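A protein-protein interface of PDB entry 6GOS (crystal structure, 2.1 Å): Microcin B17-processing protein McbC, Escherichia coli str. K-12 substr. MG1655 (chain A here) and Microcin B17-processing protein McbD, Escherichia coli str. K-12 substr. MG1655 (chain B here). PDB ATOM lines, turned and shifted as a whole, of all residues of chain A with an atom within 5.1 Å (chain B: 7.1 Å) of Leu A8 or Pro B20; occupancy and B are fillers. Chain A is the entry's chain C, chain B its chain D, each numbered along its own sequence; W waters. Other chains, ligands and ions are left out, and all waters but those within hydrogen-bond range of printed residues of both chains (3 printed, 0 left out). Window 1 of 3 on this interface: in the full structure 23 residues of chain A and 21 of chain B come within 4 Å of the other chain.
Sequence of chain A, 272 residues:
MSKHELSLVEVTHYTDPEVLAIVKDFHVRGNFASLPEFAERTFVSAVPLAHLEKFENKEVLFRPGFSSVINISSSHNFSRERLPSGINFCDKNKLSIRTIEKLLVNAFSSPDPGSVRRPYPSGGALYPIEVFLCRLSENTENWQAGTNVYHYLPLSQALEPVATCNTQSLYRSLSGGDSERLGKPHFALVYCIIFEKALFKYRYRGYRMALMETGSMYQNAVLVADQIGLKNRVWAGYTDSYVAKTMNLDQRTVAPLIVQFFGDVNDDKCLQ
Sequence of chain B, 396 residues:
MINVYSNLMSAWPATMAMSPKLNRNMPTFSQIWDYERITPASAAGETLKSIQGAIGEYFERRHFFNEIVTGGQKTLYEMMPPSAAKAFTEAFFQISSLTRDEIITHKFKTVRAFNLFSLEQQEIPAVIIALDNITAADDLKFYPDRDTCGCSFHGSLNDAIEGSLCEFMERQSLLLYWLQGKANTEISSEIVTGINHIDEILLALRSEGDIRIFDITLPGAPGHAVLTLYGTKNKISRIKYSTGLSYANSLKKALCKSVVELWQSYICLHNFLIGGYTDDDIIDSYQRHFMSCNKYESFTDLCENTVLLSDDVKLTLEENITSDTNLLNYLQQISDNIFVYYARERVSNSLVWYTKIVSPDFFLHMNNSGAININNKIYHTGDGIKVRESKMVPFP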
ATOM      1  N   LEU A   6       7.766  10.524 -14.389  1.00  0.00           N
ATOM      2  CA  LEU A   6       7.857   9.133 -14.804  1.00  0.00           C
ATOM      3  C   LEU A   6       7.775   8.269 -13.538  1.00  0.00           C
ATOM      4  O   LEU A   6       8.513   8.514 -12.564  1.00  0.00           O
ATOM      5  CB  LEU A   6       9.208   8.886 -15.471  1.00  0.00           C
ATOM      6  CG  LEU A   6       9.635   7.434 -15.679  1.00  0.00           C
ATOM      7  CD1 LEU A   6       8.734   6.758 -16.709  1.00  0.00           C
ATOM      8  CD2 LEU A   6      11.084   7.414 -16.112  1.00  0.00           C
ATOM      9  N   SER A   7       6.902   7.258 -13.562  1.00  0.00           N
ATOM     10  CA  SER A   7       6.802   6.296 -12.470  1.00  0.00           C
ATOM     11  C   SER A   7       7.849   5.201 -12.653  1.00  0.00           C
ATOM     12  O   SER A   7       8.010   4.661 -13.754  1.00  0.00           O
ATOM     13  CB  SER A   7       5.424   5.631 -12.437  1.00  0.00           C
ATOM     14  OG  SER A   7       5.384   4.652 -11.396  1.00  0.00           O
ATOM     15  N   LEU A   8       8.522   4.834 -11.574  1.00  0.00           N
ATOM     16  CA  LEU A   8       9.470   3.726 -11.617  1.00  0.00           C
ATOM     17  C   LEU A   8       8.804   2.357 -11.883  1.00  0.00           C
ATOM     18  O   LEU A   8       9.496   1.401 -12.240  1.00  0.00           O
ATOM     19  CB  LEU A   8      10.288   3.683 -10.322  1.00  0.00           C
ATOM     20  CG  LEU A   8      11.199   4.897 -10.194  1.00  0.00           C
ATOM     21  CD1 LEU A   8      11.788   4.967  -8.806  1.00  0.00           C
ATOM     22  CD2 LEU A   8      12.289   4.887 -11.256  1.00  0.00           C
ATOM     23  N   VAL A   9       7.480   2.268 -11.730  1.00  0.00           N
ATOM     24  CA  VAL A   9       6.752   1.030 -12.083  1.00  0.00           C
ATOM     25  C   VAL A   9       6.923   0.722 -13.577  1.00  0.00           C
ATOM     26  O   VAL A   9       7.031  -0.434 -13.950  1.00  0.00           O
ATOM     27  CB  VAL A   9       5.235   1.093 -11.728  1.00  0.00           C
ATOM     28  CG1 VAL A   9       4.546  -0.246 -12.031  1.00  0.00           C
ATOM     29  CG2 VAL A   9       5.008   1.445 -10.256  1.00  0.00           C
ATOM     30  N   GLU A  10       6.949   1.762 -14.417  1.00  0.00           N
ATOM     31  CA  GLU A  10       7.135   1.612 -15.881  1.00  0.00           C
ATOM     32  C   GLU A  10       8.535   1.134 -16.201  1.00  0.00           C
ATOM     33  O   GLU A  10       8.732   0.306 -17.098  1.00  0.00           O
ATOM     34  CB  GLU A  10       6.947   2.943 -16.620  1.00  0.00           C
ATOM     35  CG  GLU A  10       5.577   3.586 -16.495  1.00  0.00           C
ATOM     36  CD  GLU A  10       4.502   2.939 -17.357  1.00  0.00           C
ATOM     37  OE1 GLU A  10       4.774   1.950 -18.089  1.00  0.00           O
ATOM     38  OE2 GLU A  10       3.356   3.443 -17.291  1.00  0.00           O
ATOM     39  N   VAL A  11       9.508   1.711 -15.497  1.00  0.00           N
ATOM     40  CA  VAL A  11      10.901   1.346 -15.661  1.00  0.00           C
ATOM     41  C   VAL A  11      11.157  -0.118 -15.299  1.00  0.00           C
ATOM     42  O   VAL A  11      11.836  -0.821 -16.042  1.00  0.00           O
ATOM     43  CB  VAL A  11      11.839   2.283 -14.859  1.00  0.00           C
ATOM     44  CG1 VAL A  11      13.279   1.770 -14.875  1.00  0.00           C
ATOM     45  CG2 VAL A  11      11.793   3.676 -15.445  1.00  0.00           C
ATOM     46  N   THR A  12      10.607  -0.575 -14.177  1.00  0.00           N
ATOM     47  CA  THR A  12      10.895  -1.938 -13.693  1.00  0.00           C
ATOM     48  C   THR A  12      10.351  -3.034 -14.612  1.00  0.00           C
ATOM     49  O   THR A  12      10.859  -4.162 -14.609  1.00  0.00           O
ATOM     50  CB  THR A  12      10.436  -2.167 -12.235  1.00  0.00           C
ATOM     51  OG1 THR A  12      11.153  -3.278 -11.702  1.00  0.00           O
ATOM     52  CG2 THR A  12       8.860  -2.384 -12.098  1.00  0.00           C
ATOM     53  N   ILE A 194      19.744   5.982  -9.608  1.00  0.00           N
ATOM     54  CA  ILE A 194      18.594   5.081  -9.498  1.00  0.00           C
ATOM     55  C   ILE A 194      18.971   3.903 -10.358  1.00  0.00           C
ATOM     56  O   ILE A 194      19.022   4.024 -11.593  1.00  0.00           O
ATOM     57  CB  ILE A 194      17.286   5.720  -9.993  1.00  0.00           C
ATOM     58  CG1 ILE A 194      16.939   6.947  -9.146  1.00  0.00           C
ATOM     59  CG2 ILE A 194      16.125   4.720  -9.897  1.00  0.00           C
ATOM     60  CD1 ILE A 194      15.752   7.712  -9.698  1.00  0.00           C
ATOM     61  N   GLU A 196      17.769   0.976 -11.399  1.00  0.00           N
ATOM     62  CA  GLU A 196      16.937   0.438 -12.481  1.00  0.00           C
ATOM     63  C   GLU A 196      16.755   1.407 -13.638  1.00  0.00           C
ATOM     64  O   GLU A 196      16.650   0.991 -14.793  1.00  0.00           O
ATOM     65  CB  GLU A 196      15.596  -0.100 -11.947  1.00  0.00           C
ATOM     66  CG  GLU A 196      15.789  -1.406 -11.177  1.00  0.00           C
ATOM     67  CD  GLU A 196      14.485  -2.081 -10.773  1.00  0.00           C
ATOM     68  OE1 GLU A 196      13.642  -2.305 -11.666  1.00  0.00           O
ATOM     69  OE2 GLU A 196      14.318  -2.412  -9.562  1.00  0.00           O
ATOM     70  N   LYS A 197      16.792   2.697 -13.351  1.00  0.00           N
ATOM     71  CA  LYS A 197      16.773   3.695 -14.421  1.00  0.00           C
ATOM     72  C   LYS A 197      18.072   3.661 -15.238  1.00  0.00           C
ATOM     73  O   LYS A 197      18.060   3.847 -16.448  1.00  0.00           O
ATOM     74  CB  LYS A 197      16.588   5.062 -13.805  1.00  0.00           C
ATOM     75  CG  LYS A 197      16.306   6.149 -14.789  1.00  0.00           C
ATOM     76  CD  LYS A 197      14.848   6.338 -15.033  1.00  0.00           C
ATOM     77  CE  LYS A 197      14.657   7.702 -15.666  1.00  0.00           C
ATOM     78  NZ  LYS A 197      14.727   7.629 -17.149  1.00  0.00           N
ATOM     79  N   THR A 253      16.843   0.894  -4.235  1.00  0.00           N
ATOM     80  CA  THR A 253      16.558   1.603  -5.468  1.00  0.00           C
ATOM     81  C   THR A 253      17.601   2.633  -5.857  1.00  0.00           C
ATOM     82  O   THR A 253      17.888   2.794  -7.051  1.00  0.00           O
ATOM     83  CB  THR A 253      15.217   2.322  -5.274  1.00  0.00           C
ATOM     84  OG1 THR A 253      14.193   1.328  -5.153  1.00  0.00           O
ATOM     85  CG2 THR A 253      14.877   3.238  -6.410  1.00  0.00           C
ATOM     86  N   MET B   1      12.400  -4.503  -9.267  1.00  0.00           N
ATOM     87  CA  MET B   1      12.906  -5.662  -8.448  1.00  0.00           C
ATOM     88  C   MET B   1      11.976  -6.841  -8.568  1.00  0.00           C
ATOM     89  O   MET B   1      10.813  -6.695  -9.013  1.00  0.00           O
ATOM     90  CB  MET B   1      13.117  -5.274  -6.996  1.00  0.00           C
ATOM     91  CG  MET B   1      14.476  -4.609  -6.781  1.00  0.00           C
ATOM     92  SD  MET B   1      14.585  -3.738  -5.222  1.00  0.00           S
ATOM     93  CE  MET B   1      13.596  -2.272  -5.576  1.00  0.00           C
ATOM     94  N   ASN B   3      11.112  -9.086 -10.651  1.00  0.00           N
ATOM     95  CA  ASN B   3      11.147  -9.165 -12.108  1.00  0.00           C
ATOM     96  C   ASN B   3      11.221 -10.614 -12.626  1.00  0.00           C
ATOM     97  O   ASN B   3      12.162 -10.998 -13.285  1.00  0.00           O
ATOM     98  CB  ASN B   3      12.258  -8.279 -12.654  1.00  0.00           C
ATOM     99  CG  ASN B   3      12.095  -6.823 -12.252  1.00  0.00           C
ATOM    100  OD1 ASN B   3      12.890  -6.288 -11.480  1.00  0.00           O
ATOM    101  ND2 ASN B   3      11.050  -6.177 -12.753  1.00  0.00           N
ATOM    102  N   ALA B  17       6.596  -7.897 -10.495  1.00  0.00           N
ATOM    103  CA  ALA B  17       7.599  -6.905 -10.132  1.00  0.00           C
ATOM    104  C   ALA B  17       7.272  -6.193  -8.840  1.00  0.00           C
ATOM    105  O   ALA B  17       6.117  -5.917  -8.542  1.00  0.00           O
ATOM    106  CB  ALA B  17       7.797  -5.895 -11.253  1.00  0.00           C
ATOM    107  N   MET B  18       8.314  -5.938  -8.059  1.00  0.00           N
ATOM    108  CA  MET B  18       8.256  -5.032  -6.928  1.00  0.00           C
ATOM    109  C   MET B  18       8.838  -3.745  -7.460  1.00  0.00           C
ATOM    110  O   MET B  18       9.932  -3.728  -8.005  1.00  0.00           O
ATOM    111  CB  MET B  18       9.082  -5.572  -5.759  1.00  0.00           C
ATOM    112  CG  MET B  18       9.101  -4.716  -4.497  1.00  0.00           C
ATOM    113  SD  MET B  18      10.248  -5.407  -3.270  1.00  0.00           S
ATOM    114  CE  MET B  18      11.725  -4.458  -3.546  1.00  0.00           C
ATOM    115  N   SER B  19       8.110  -2.659  -7.280  1.00  0.00           N
ATOM    116  CA  SER B  19       8.477  -1.398  -7.872  1.00  0.00           C
ATOM    117  C   SER B  19       9.574  -0.701  -7.043  1.00  0.00           C
ATOM    118  O   SER B  19       9.465  -0.638  -5.828  1.00  0.00           O
ATOM    119  CB  SER B  19       7.232  -0.512  -7.969  1.00  0.00           C
ATOM    120  OG  SER B  19       7.591   0.707  -8.562  1.00  0.00           O
ATOM    121  N   PRO B  20      10.626  -0.172  -7.696  1.00  0.00           N
ATOM    122  CA  PRO B  20      11.533   0.701  -6.951  1.00  0.00           C
ATOM    123  C   PRO B  20      10.827   1.967  -6.481  1.00  0.00           C
ATOM    124  O   PRO B  20       9.818   2.367  -7.063  1.00  0.00           O
ATOM    125  CB  PRO B  20      12.641   1.065  -7.957  1.00  0.00           C
ATOM    126  CG  PRO B  20      12.328   0.382  -9.220  1.00  0.00           C
ATOM    127  CD  PRO B  20      11.022  -0.340  -9.105  1.00  0.00           C
ATOM    128  N   LYS B  21      11.371   2.562  -5.430  1.00  0.00           N
ATOM    129  CA  LYS B  21      10.904   3.817  -4.882  1.00  0.00           C
ATOM    130  C   LYS B  21      12.124   4.556  -4.287  1.00  0.00           C
ATOM    131  O   LYS B  21      13.049   3.922  -3.747  1.00  0.00           O
ATOM    132  CB  LYS B  21       9.799   3.538  -3.845  1.00  0.00           C
ATOM    133  CG  LYS B  21      10.328   2.890  -2.590  1.00  0.00           C
ATOM    134  CD  LYS B  21       9.334   2.081  -1.793  1.00  0.00           C
ATOM    135  CE  LYS B  21       9.870   1.980  -0.377  1.00  0.00           C
ATOM    136  NZ  LYS B  21       9.459   0.748   0.310  1.00  0.00           N
ATOM    137  N   LEU B  22      12.160   5.876  -4.414  1.00  0.00           N
ATOM    138  CA  LEU B  22      13.228   6.639  -3.816  1.00  0.00           C
ATOM    139  C   LEU B  22      13.102   6.672  -2.300  1.00  0.00           C
ATOM    140  O   LEU B  22      14.109   6.648  -1.615  1.00  0.00           O
ATOM    141  CB  LEU B  22      13.274   8.068  -4.345  1.00  0.00           C
ATOM    142  CG  LEU B  22      13.559   8.327  -5.822  1.00  0.00           C
ATOM    143  CD1 LEU B  22      13.636   9.825  -6.078  1.00  0.00           C
ATOM    144  CD2 LEU B  22      14.832   7.639  -6.253  1.00  0.00           C
ATOM    145  N   ASN B  23      11.875   6.703  -1.783  1.00  0.00           N
ATOM    146  CA  ASN B  23      11.618   7.053  -0.376  1.00  0.00           C
ATOM    147  C   ASN B  23      11.442   5.789   0.461  1.00  0.00           C
ATOM    148  O   ASN B  23      10.486   5.037   0.252  1.00  0.00           O
ATOM    149  CB  ASN B  23      10.354   7.930  -0.309  1.00  0.00           C
ATOM    150  CG  ASN B  23      10.016   8.408   1.090  1.00  0.00           C
ATOM    151  OD1 ASN B  23      10.582   7.958   2.094  1.00  0.00           O
ATOM    152  ND2 ASN B  23       9.054   9.320   1.161  1.00  0.00           N
ATOM    153  N   PHE B  29       5.144  -1.198  -3.418  1.00  0.00           N
ATOM    154  CA  PHE B  29       4.066  -1.549  -4.334  1.00  0.00           C
ATOM    155  C   PHE B  29       4.558  -2.703  -5.199  1.00  0.00           C
ATOM    156  O   PHE B  29       5.632  -2.606  -5.817  1.00  0.00           O
ATOM    157  CB  PHE B  29       3.728  -0.338  -5.198  1.00  0.00           C
ATOM    158  CG  PHE B  29       2.673  -0.608  -6.212  1.00  0.00           C
ATOM    159  CD1 PHE B  29       1.323  -0.543  -5.864  1.00  0.00           C
ATOM    160  CD2 PHE B  29       3.012  -0.961  -7.526  1.00  0.00           C
ATOM    161  CE1 PHE B  29       0.333  -0.809  -6.816  1.00  0.00           C
ATOM    162  CE2 PHE B  29       2.025  -1.216  -8.475  1.00  0.00           C
ATOM    163  CZ  PHE B  29       0.680  -1.144  -8.114  1.00  0.00           C
ATOM    164  N   ASN B 271      -0.873   6.826 -11.986  1.00  0.00           N
ATOM    165  CA  ASN B 271       0.064   6.277 -12.971  1.00  0.00           C
ATOM    166  C   ASN B 271      -0.590   5.930 -14.324  1.00  0.00           C
ATOM    167  O   ASN B 271       0.011   6.105 -15.397  1.00  0.00           O
ATOM    168  CB  ASN B 271       0.803   5.074 -12.386  1.00  0.00           C
ATOM    169  CG  ASN B 271       1.893   5.483 -11.390  1.00  0.00           C
ATOM    170  OD1 ASN B 271       2.322   6.648 -11.354  1.00  0.00           O
ATOM    171  ND2 ASN B 271       2.354   4.521 -10.586  1.00  0.00           N
HETATM  172  O   HOH W   1       2.797   5.557 -15.582  1.00  0.00           O
HETATM  173  O   HOH W   2       9.064  -7.004 -14.562  1.00  0.00           O
HETATM  174  O   HOH W   3       4.919   5.976  -9.131  1.00  0.00           O
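Leu A8 touches two residues of chain B. Of the printed residues of chain B, Thr A253 touches Met B1 (3.7 Å), Pro B20 (3.2 Å) and Lys B21 (3.1 Å). Printed residues of chain B within 4 Å of Glu A196: Met B1 and Pro B20. Of the printed residues of chain A, Leu B22 touches Ile A194. Printed residues of chain A within 4 Å of Lys B21: Thr A253. Printed residues of chain A within 4 Å of Asn B3: Thr A12. Val A11 touches none of the printed residues of chain B. The nearest residue of chain B that does not touch Leu A8 is Lys B21 (4.2 Å). The nearest printed residue of chain A that does not touch Pro B20 is Val A9 (5.1 Å).
OG of Ser A7 is in hydrogen-bond range of ND2 of Asn B271. O of Thr A12 lies within hydrogen-bond range of ND2 of Asn B3 (2.7 Å). The backbone NH (N) of Lys B21 sits at hydrogen-bond distance from the side-chain hydroxyl (OG1) of Thr A253 (3.1 Å). The side-chain carboxylate of Glu A196 sits at hydrogen-bond distance from the backbone NH of Met B1 (2.9 Å). The side-chain hydroxyl (OG1) of Thr A12 is in hydrogen-bond range of the backbone NH (N) of Met B1 (3.0 Å).
The backbone NH (N) of Met B18 sits at hydrogen-bond distance from the backbone carbonyl oxygen (O) of Met B1 (2.8 Å). OG of Ser A7 sits close to N of Val A9, at 3.2 Å. The side-chain hydroxyl (OG1) of Thr A12 lies within hydrogen-bond range of the side-chain carboxylate (OE1) of Glu A196. The side-chain amide oxygen (OD1) of Asn B3 lies within hydrogen-bond range of the backbone NH (N) of Met B1 (2.9 Å). The backbone NH (N) of Ser B19 sits at hydrogen-bond distance from the backbone carbonyl oxygen (O) of Phe B29 (2.9 Å).
Water W3 lies within hydrogen-bond range of OG of Ser A7 (2.7 Å) and ND2 of Asn B271 (3.3 Å). Water W1 lies within hydrogen-bond range of the side-chain carboxylate (OE2) of Glu A10 and the backbone carbonyl oxygen (O) of Asn B271. Water W2 bridges ND2 of Asn B3 (2.8 Å) and O of Thr A12 (3.4 Å).
Leu A8 touches Ser B19 (C to OG, 3.9 Å). O of Pro B20 touches CB of Leu A8 (3.5 Å). OG of Ser B19 touches CG2 of Val A9, at 3.2 Å. Thr A12 touches Ala B17 (CG2 to CB, 3.8 Å). OG1 of Thr A12 touches O of Met B18, 3.9 Å away. Thr A12 touches Pro B20. Leu B22 touches Ile A194. Glu A196 touches Pro B20 (OE2 to CG, 3.4 Å). Thr A253 touches Met B1. OG1 of Thr A253 touches CB of Pro B20 (3.2 Å).
Printed residues of chain A that touch a printed residue of chain B: Ser A7, Leu A8, Val A9, Thr A12, Ile A194, Glu A196 and Thr A253. Hydrophobic or aromatic side chains of chain A within 4 Å of the printed part of chain B: Leu A8, Val A9 and Ile A194. Along chain A the printed residues that touch a printed residue of chain B span positions 7 to 253. Printed residues of chain B that touch a printed residue of chain A: Met B1, Asn B3, Ala B17, Met B18, Ser B19, Pro B20, Lys B21, Leu B22 and Asn B271. Among the printed residues, no Asp or Glu carboxylate lies within 4 Å of a Lys or Arg side-chain nitrogen of the other chain.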
